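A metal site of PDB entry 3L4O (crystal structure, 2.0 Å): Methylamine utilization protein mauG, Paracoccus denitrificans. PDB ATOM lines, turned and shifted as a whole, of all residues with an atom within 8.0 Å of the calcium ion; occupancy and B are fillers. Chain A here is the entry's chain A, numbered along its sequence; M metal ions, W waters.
Three residues have an atom within 4 Å of the calcium ion: Asn 66, Thr 275 and Pro 277. The nearest printed residue that does not touch the calcium ion is Gly 276 (4.1 Å).
The calcium ion is bound by water W2 (2.3 Å), the backbone carbonyl oxygen of Thr 275 (2.3 Å), water W3 (2.4 Å), the side-chain amide oxygen of Asn 66 (2.4 Å), the backbone carbonyl oxygen of Pro 277 (2.4 Å), water W4 (2.6 Å) and water W1 (2.7 Å).
Water W1 lies within hydrogen-bond range of O of Gly 276 (2.8 Å), NH2 of Arg 39 (3.2 Å) and ND2 of Asn 66 (3.3 Å).
O of Asn 66 is in hydrogen-bond range of NE1 of Trp 93 (2.8 Å). The side-chain hydroxyl (OG1) of Thr 275 lies close to the backbone carbonyl oxygen (O) of Asn 271 (3.3 Å). The side-chain amide nitrogen (ND2) of Asn 66 is in hydrogen-bond range of the backbone carbonyl oxygen (O) of Ala 52. The backbone NH (N) of Asn 66 lies within hydrogen-bond range of the backbone carbonyl oxygen (O) of His 280 (2.8 Å). The backbone carbonyl oxygen (O) of Leu 51 lies within hydrogen-bond range of the side-chain amide nitrogen (ND2) of Asn 66 (3.2 Å).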
ATOM      1  N   ARG A  39       1.520 -22.025  39.848  1.00  0.00           N
ATOM      2  CA  ARG A  39       0.751 -21.885  38.598  1.00  0.00           C
ATOM      3  C   ARG A  39      -0.081 -23.147  38.357  1.00  0.00           C
ATOM      4  O   ARG A  39      -0.183 -23.661  37.248  1.00  0.00           O
ATOM      5  CB  ARG A  39       1.638 -21.580  37.333  1.00  0.00           C
ATOM      6  CG  ARG A  39       0.826 -20.760  36.241  1.00  0.00           C
ATOM      7  CD  ARG A  39       1.532 -20.075  35.030  1.00  0.00           C
ATOM      8  NE  ARG A  39       1.170 -20.941  34.031  1.00  0.00           N
ATOM      9  CZ  ARG A  39       0.503 -20.740  32.903  1.00  0.00           C
ATOM     10  NH1 ARG A  39       0.192 -19.571  32.349  1.00  0.00           N
ATOM     11  NH2 ARG A  39       0.259 -21.869  32.288  1.00  0.00           N
ATOM     12  N   THR A  42       1.674 -26.070  36.538  1.00  0.00           N
ATOM     13  CA  THR A  42       2.061 -25.980  35.110  1.00  0.00           C
ATOM     14  C   THR A  42       3.252 -25.000  35.011  1.00  0.00           C
ATOM     15  O   THR A  42       3.752 -24.480  36.035  1.00  0.00           O
ATOM     16  CB  THR A  42       0.914 -25.414  34.257  1.00  0.00           C
ATOM     17  OG1 THR A  42       0.594 -24.079  34.745  1.00  0.00           O
ATOM     18  CG2 THR A  42      -0.271 -26.287  34.292  1.00  0.00           C
ATOM     19  N   ASP A  43       3.696 -24.786  33.769  1.00  0.00           N
ATOM     20  CA  ASP A  43       4.969 -24.117  33.477  1.00  0.00           C
ATOM     21  C   ASP A  43       4.790 -22.641  33.125  1.00  0.00           C
ATOM     22  O   ASP A  43       4.272 -22.305  32.025  1.00  0.00           O
ATOM     23  CB  ASP A  43       5.698 -24.831  32.328  1.00  0.00           C
ATOM     24  CG  ASP A  43       7.190 -24.407  32.203  1.00  0.00           C
ATOM     25  OD1 ASP A  43       7.869 -25.061  31.389  1.00  0.00           O
ATOM     26  OD2 ASP A  43       7.678 -23.426  32.899  1.00  0.00           O
ATOM     27  N   LEU A  51       4.530 -20.089  25.915  1.00  0.00           N
ATOM     28  CA  LEU A  51       4.308 -21.080  26.982  1.00  0.00           C
ATOM     29  C   LEU A  51       3.763 -22.413  26.435  1.00  0.00           C
ATOM     30  O   LEU A  51       3.341 -23.288  27.214  1.00  0.00           O
ATOM     31  CB  LEU A  51       3.380 -20.535  28.088  1.00  0.00           C
ATOM     32  CG  LEU A  51       3.911 -19.645  29.242  1.00  0.00           C
ATOM     33  CD1 LEU A  51       4.782 -18.558  28.765  1.00  0.00           C
ATOM     34  CD2 LEU A  51       2.732 -19.017  30.016  1.00  0.00           C
ATOM     35  N   ALA A  52       3.795 -22.578  25.099  1.00  0.00           N
ATOM     36  CA  ALA A  52       3.195 -23.758  24.462  1.00  0.00           C
ATOM     37  C   ALA A  52       3.875 -25.054  24.900  1.00  0.00           C
ATOM     38  O   ALA A  52       3.185 -26.042  25.119  1.00  0.00           O
ATOM     39  CB  ALA A  52       3.194 -23.667  22.891  1.00  0.00           C
ATOM     40  N   ASN A  66       2.172 -29.496  25.479  1.00  0.00           N
ATOM     41  CA  ASN A  66       2.044 -28.538  26.573  1.00  0.00           C
ATOM     42  C   ASN A  66       2.075 -29.263  27.920  1.00  0.00           C
ATOM     43  O   ASN A  66       1.441 -30.372  28.099  1.00  0.00           O
ATOM     44  CB  ASN A  66       0.691 -27.845  26.391  1.00  0.00           C
ATOM     45  CG  ASN A  66       0.446 -26.755  27.408  1.00  0.00           C
ATOM     46  OD1 ASN A  66      -0.499 -26.859  28.239  1.00  0.00           O
ATOM     47  ND2 ASN A  66       1.325 -25.728  27.411  1.00  0.00           N
ATOM     48  N   THR A  67       2.795 -28.691  28.878  1.00  0.00           N
ATOM     49  CA  THR A  67       2.833 -29.284  30.251  1.00  0.00           C
ATOM     50  C   THR A  67       1.440 -29.187  30.973  1.00  0.00           C
ATOM     51  O   THR A  67       0.964 -28.060  31.247  1.00  0.00           O
ATOM     52  CB  THR A  67       3.942 -28.656  31.129  1.00  0.00           C
ATOM     53  OG1 THR A  67       5.226 -28.849  30.515  1.00  0.00           O
ATOM     54  CG2 THR A  67       3.988 -29.288  32.511  1.00  0.00           C
ATOM     55  N   PRO A  68       0.778 -30.347  31.301  1.00  0.00           N
ATOM     56  CA  PRO A  68      -0.553 -30.255  31.918  1.00  0.00           C
ATOM     57  C   PRO A  68      -0.475 -30.086  33.451  1.00  0.00           C
ATOM     58  O   PRO A  68       0.516 -30.457  34.113  1.00  0.00           O
ATOM     59  CB  PRO A  68      -1.203 -31.610  31.546  1.00  0.00           C
ATOM     60  CG  PRO A  68      -0.066 -32.514  31.804  1.00  0.00           C
ATOM     61  CD  PRO A  68       1.147 -31.763  31.106  1.00  0.00           C
ATOM     62  N   THR A  69      -1.554 -29.596  34.055  1.00  0.00           N
ATOM     63  CA  THR A  69      -1.654 -29.615  35.538  1.00  0.00           C
ATOM     64  C   THR A  69      -1.558 -30.975  36.181  1.00  0.00           C
ATOM     65  O   THR A  69      -1.994 -31.957  35.595  1.00  0.00           O
ATOM     66  CB  THR A  69      -2.986 -28.938  36.052  1.00  0.00           C
ATOM     67  OG1 THR A  69      -2.957 -28.846  37.495  1.00  0.00           O
ATOM     68  CG2 THR A  69      -4.252 -29.703  35.611  1.00  0.00           C
ATOM     69  N   TRP A  93      -0.991 -36.891  27.707  1.00  0.00           N
ATOM     70  CA  TRP A  93      -2.050 -36.519  26.766  1.00  0.00           C
ATOM     71  C   TRP A  93      -2.402 -37.688  25.879  1.00  0.00           C
ATOM     72  O   TRP A  93      -3.516 -37.734  25.326  1.00  0.00           O
ATOM     73  CB  TRP A  93      -1.637 -35.350  25.891  1.00  0.00           C
ATOM     74  CG  TRP A  93      -1.529 -33.992  26.553  1.00  0.00           C
ATOM     75  CD1 TRP A  93      -0.383 -33.382  26.966  1.00  0.00           C
ATOM     76  CD2 TRP A  93      -2.585 -33.027  26.740  1.00  0.00           C
ATOM     77  NE1 TRP A  93      -0.665 -32.125  27.463  1.00  0.00           N
ATOM     78  CE2 TRP A  93      -2.009 -31.890  27.346  1.00  0.00           C
ATOM     79  CE3 TRP A  93      -3.958 -33.032  26.478  1.00  0.00           C
ATOM     80  CZ2 TRP A  93      -2.738 -30.738  27.655  1.00  0.00           C
ATOM     81  CZ3 TRP A  93      -4.714 -31.870  26.802  1.00  0.00           C
ATOM     82  CH2 TRP A  93      -4.090 -30.753  27.385  1.00  0.00           C
ATOM     83  N   ASN A 271      -9.128 -25.670  37.186  1.00  0.00           N
ATOM     84  CA  ASN A 271      -8.012 -24.685  37.050  1.00  0.00           C
ATOM     85  C   ASN A 271      -7.761 -24.218  35.610  1.00  0.00           C
ATOM     86  O   ASN A 271      -6.739 -23.548  35.304  1.00  0.00           O
ATOM     87  CB  ASN A 271      -6.753 -25.229  37.721  1.00  0.00           C
ATOM     88  CG  ASN A 271      -6.909 -25.295  39.276  1.00  0.00           C
ATOM     89  OD1 ASN A 271      -7.402 -24.318  39.881  1.00  0.00           O
ATOM     90  ND2 ASN A 271      -6.486 -26.415  39.910  1.00  0.00           N
ATOM     91  N   VAL A 272      -8.695 -24.532  34.710  1.00  0.00           N
ATOM     92  CA  VAL A 272      -8.452 -24.264  33.298  1.00  0.00           C
ATOM     93  C   VAL A 272      -8.132 -22.743  33.126  1.00  0.00           C
ATOM     94  O   VAL A 272      -7.285 -22.371  32.294  1.00  0.00           O
ATOM     95  CB  VAL A 272      -9.601 -24.775  32.395  1.00  0.00           C
ATOM     96  CG1 VAL A 272     -10.864 -23.965  32.610  1.00  0.00           C
ATOM     97  CG2 VAL A 272      -9.235 -24.787  30.941  1.00  0.00           C
ATOM     98  N   VAL A 274      -6.409 -20.674  34.786  1.00  0.00           N
ATOM     99  CA  VAL A 274      -5.063 -20.226  35.099  1.00  0.00           C
ATOM    100  C   VAL A 274      -3.961 -21.110  34.427  1.00  0.00           C
ATOM    101  O   VAL A 274      -2.769 -20.929  34.686  1.00  0.00           O
ATOM    102  CB  VAL A 274      -4.920 -20.094  36.636  1.00  0.00           C
ATOM    103  CG1 VAL A 274      -6.005 -19.177  37.191  1.00  0.00           C
ATOM    104  CG2 VAL A 274      -4.934 -21.443  37.331  1.00  0.00           C
ATOM    105  N   THR A 275      -4.333 -22.028  33.539  1.00  0.00           N
ATOM    106  CA  THR A 275      -3.329 -22.996  33.008  1.00  0.00           C
ATOM    107  C   THR A 275      -3.165 -22.899  31.472  1.00  0.00           C
ATOM    108  O   THR A 275      -2.854 -23.905  30.807  1.00  0.00           O
ATOM    109  CB  THR A 275      -3.609 -24.462  33.408  1.00  0.00           C
ATOM    110  OG1 THR A 275      -4.889 -24.872  32.887  1.00  0.00           O
ATOM    111  CG2 THR A 275      -3.659 -24.638  34.925  1.00  0.00           C
ATOM    112  N   GLY A 276      -3.412 -21.708  30.917  1.00  0.00           N
ATOM    113  CA  GLY A 276      -3.171 -21.462  29.478  1.00  0.00           C
ATOM    114  C   GLY A 276      -1.683 -21.560  29.175  1.00  0.00           C
ATOM    115  O   GLY A 276      -0.872 -21.469  30.086  1.00  0.00           O
ATOM    116  N   PRO A 277      -1.308 -21.692  27.877  1.00  0.00           N
ATOM    117  CA  PRO A 277      -2.150 -21.780  26.705  1.00  0.00           C
ATOM    118  C   PRO A 277      -2.797 -23.184  26.663  1.00  0.00           C
ATOM    119  O   PRO A 277      -2.447 -24.064  27.487  1.00  0.00           O
ATOM    120  CB  PRO A 277      -1.159 -21.596  25.531  1.00  0.00           C
ATOM    121  CG  PRO A 277       0.143 -22.016  26.090  1.00  0.00           C
ATOM    122  CD  PRO A 277       0.124 -21.893  27.556  1.00  0.00           C
ATOM    123  N   TYR A 278      -3.735 -23.389  25.743  1.00  0.00           N
ATOM    124  CA  TYR A 278      -4.619 -24.563  25.806  1.00  0.00           C
ATOM    125  C   TYR A 278      -4.379 -25.626  24.745  1.00  0.00           C
ATOM    126  O   TYR A 278      -3.834 -25.337  23.689  1.00  0.00           O
ATOM    127  CB  TYR A 278      -6.055 -24.045  25.757  1.00  0.00           C
ATOM    128  CG  TYR A 278      -6.231 -23.132  26.943  1.00  0.00           C
ATOM    129  CD1 TYR A 278      -6.218 -21.737  26.807  1.00  0.00           C
ATOM    130  CD2 TYR A 278      -6.359 -23.666  28.228  1.00  0.00           C
ATOM    131  CE1 TYR A 278      -6.332 -20.906  27.958  1.00  0.00           C
ATOM    132  CE2 TYR A 278      -6.539 -22.838  29.349  1.00  0.00           C
ATOM    133  CZ  TYR A 278      -6.489 -21.471  29.219  1.00  0.00           C
ATOM    134  OH  TYR A 278      -6.625 -20.671  30.352  1.00  0.00           O
ATOM    135  N   MET A 279      -4.911 -26.828  25.000  1.00  0.00           N
ATOM    136  CA  MET A 279      -4.789 -27.984  24.105  1.00  0.00           C
ATOM    137  C   MET A 279      -3.436 -28.686  24.287  1.00  0.00           C
ATOM    138  O   MET A 279      -2.524 -28.175  24.991  1.00  0.00           O
ATOM    139  CB  MET A 279      -5.113 -27.625  22.645  1.00  0.00           C
ATOM    140  CG  MET A 279      -6.549 -26.923  22.484  1.00  0.00           C
ATOM    141  SD  MET A 279      -7.945 -27.918  23.221  1.00  0.00           S
ATOM    142  CE  MET A 279      -9.214 -26.695  22.997  1.00  0.00           C
ATOM    143  N   HIS A 280      -3.331 -29.855  23.665  1.00  0.00           N
ATOM    144  CA  HIS A 280      -2.193 -30.743  23.858  1.00  0.00           C
ATOM    145  C   HIS A 280      -0.940 -30.069  23.353  1.00  0.00           C
ATOM    146  O   HIS A 280       0.140 -30.420  23.814  1.00  0.00           O
ATOM    147  CB  HIS A 280      -2.446 -32.088  23.165  1.00  0.00           C
ATOM    148  CG  HIS A 280      -2.470 -31.983  21.666  1.00  0.00           C
ATOM    149  ND1 HIS A 280      -3.635 -32.032  20.941  1.00  0.00           N
ATOM    150  CD2 HIS A 280      -1.468 -31.842  20.764  1.00  0.00           C
ATOM    151  CE1 HIS A 280      -3.357 -31.906  19.641  1.00  0.00           C
ATOM    152  NE2 HIS A 280      -2.042 -31.847  19.514  1.00  0.00           N
ATOM    153  N   ASN A 281      -1.078 -29.077  22.454  1.00  0.00           N
ATOM    154  CA  ASN A 281       0.075 -28.391  21.865  1.00  0.00           C
ATOM    155  C   ASN A 281       0.165 -26.882  22.219  1.00  0.00           C
ATOM    156  O   ASN A 281       0.956 -26.165  21.639  1.00  0.00           O
ATOM    157  CB  ASN A 281       0.161 -28.575  20.340  1.00  0.00           C
ATOM    158  CG  ASN A 281      -1.070 -28.113  19.643  1.00  0.00           C
ATOM    159  OD1 ASN A 281      -1.910 -27.436  20.256  1.00  0.00           O
ATOM    160  ND2 ASN A 281      -1.227 -28.490  18.352  1.00  0.00           N
ATOM    161  N   GLY A 282      -0.637 -26.441  23.201  1.00  0.00           N
ATOM    162  CA  GLY A 282      -0.607 -25.039  23.639  1.00  0.00           C
ATOM    163  C   GLY A 282      -0.912 -24.045  22.547  1.00  0.00           C
ATOM    164  O   GLY A 282      -0.450 -22.906  22.602  1.00  0.00           O
ATOM    165  N   VAL A 283      -1.676 -24.471  21.534  1.00  0.00           N
ATOM    166  CA  VAL A 283      -1.841 -23.632  20.305  1.00  0.00           C
ATOM    167  C   VAL A 283      -2.643 -22.376  20.549  1.00  0.00           C
ATOM    168  O   VAL A 283      -2.473 -21.373  19.842  1.00  0.00           O
ATOM    169  CB  VAL A 283      -2.486 -24.454  19.171  1.00  0.00           C
ATOM    170  CG1 VAL A 283      -3.899 -25.049  19.578  1.00  0.00           C
ATOM    171  CG2 VAL A 283      -2.566 -23.632  17.936  1.00  0.00           C
ATOM    172  N   PHE A 284      -3.488 -22.375  21.563  1.00  0.00           N
ATOM    173  CA  PHE A 284      -4.299 -21.197  21.842  1.00  0.00           C
ATOM    174  C   PHE A 284      -3.927 -20.609  23.200  1.00  0.00           C
ATOM    175  O   PHE A 284      -4.062 -21.281  24.210  1.00  0.00           O
ATOM    176  CB  PHE A 284      -5.821 -21.548  21.886  1.00  0.00           C
ATOM    177  CG  PHE A 284      -6.335 -22.328  20.717  1.00  0.00           C
ATOM    178  CD1 PHE A 284      -6.014 -21.982  19.407  1.00  0.00           C
ATOM    179  CD2 PHE A 284      -7.229 -23.392  20.938  1.00  0.00           C
ATOM    180  CE1 PHE A 284      -6.518 -22.704  18.361  1.00  0.00           C
ATOM    181  CE2 PHE A 284      -7.756 -24.085  19.885  1.00  0.00           C
ATOM    182  CZ  PHE A 284      -7.397 -23.766  18.594  1.00  0.00           C
HETATM  183 CA    CA M   1      -2.217 -25.604  29.347  1.00  0.00          CA
HETATM  184  O   HOH W   1      -0.049 -24.166  30.034  1.00  0.00           O
HETATM  185  O   HOH W   2      -1.540 -26.846  31.112  1.00  0.00           O
HETATM  186  O   HOH W   3      -4.389 -25.960  30.218  1.00  0.00           O
HETATM  187  O   HOH W   4      -3.335 -27.410  27.922  1.00  0.00           O
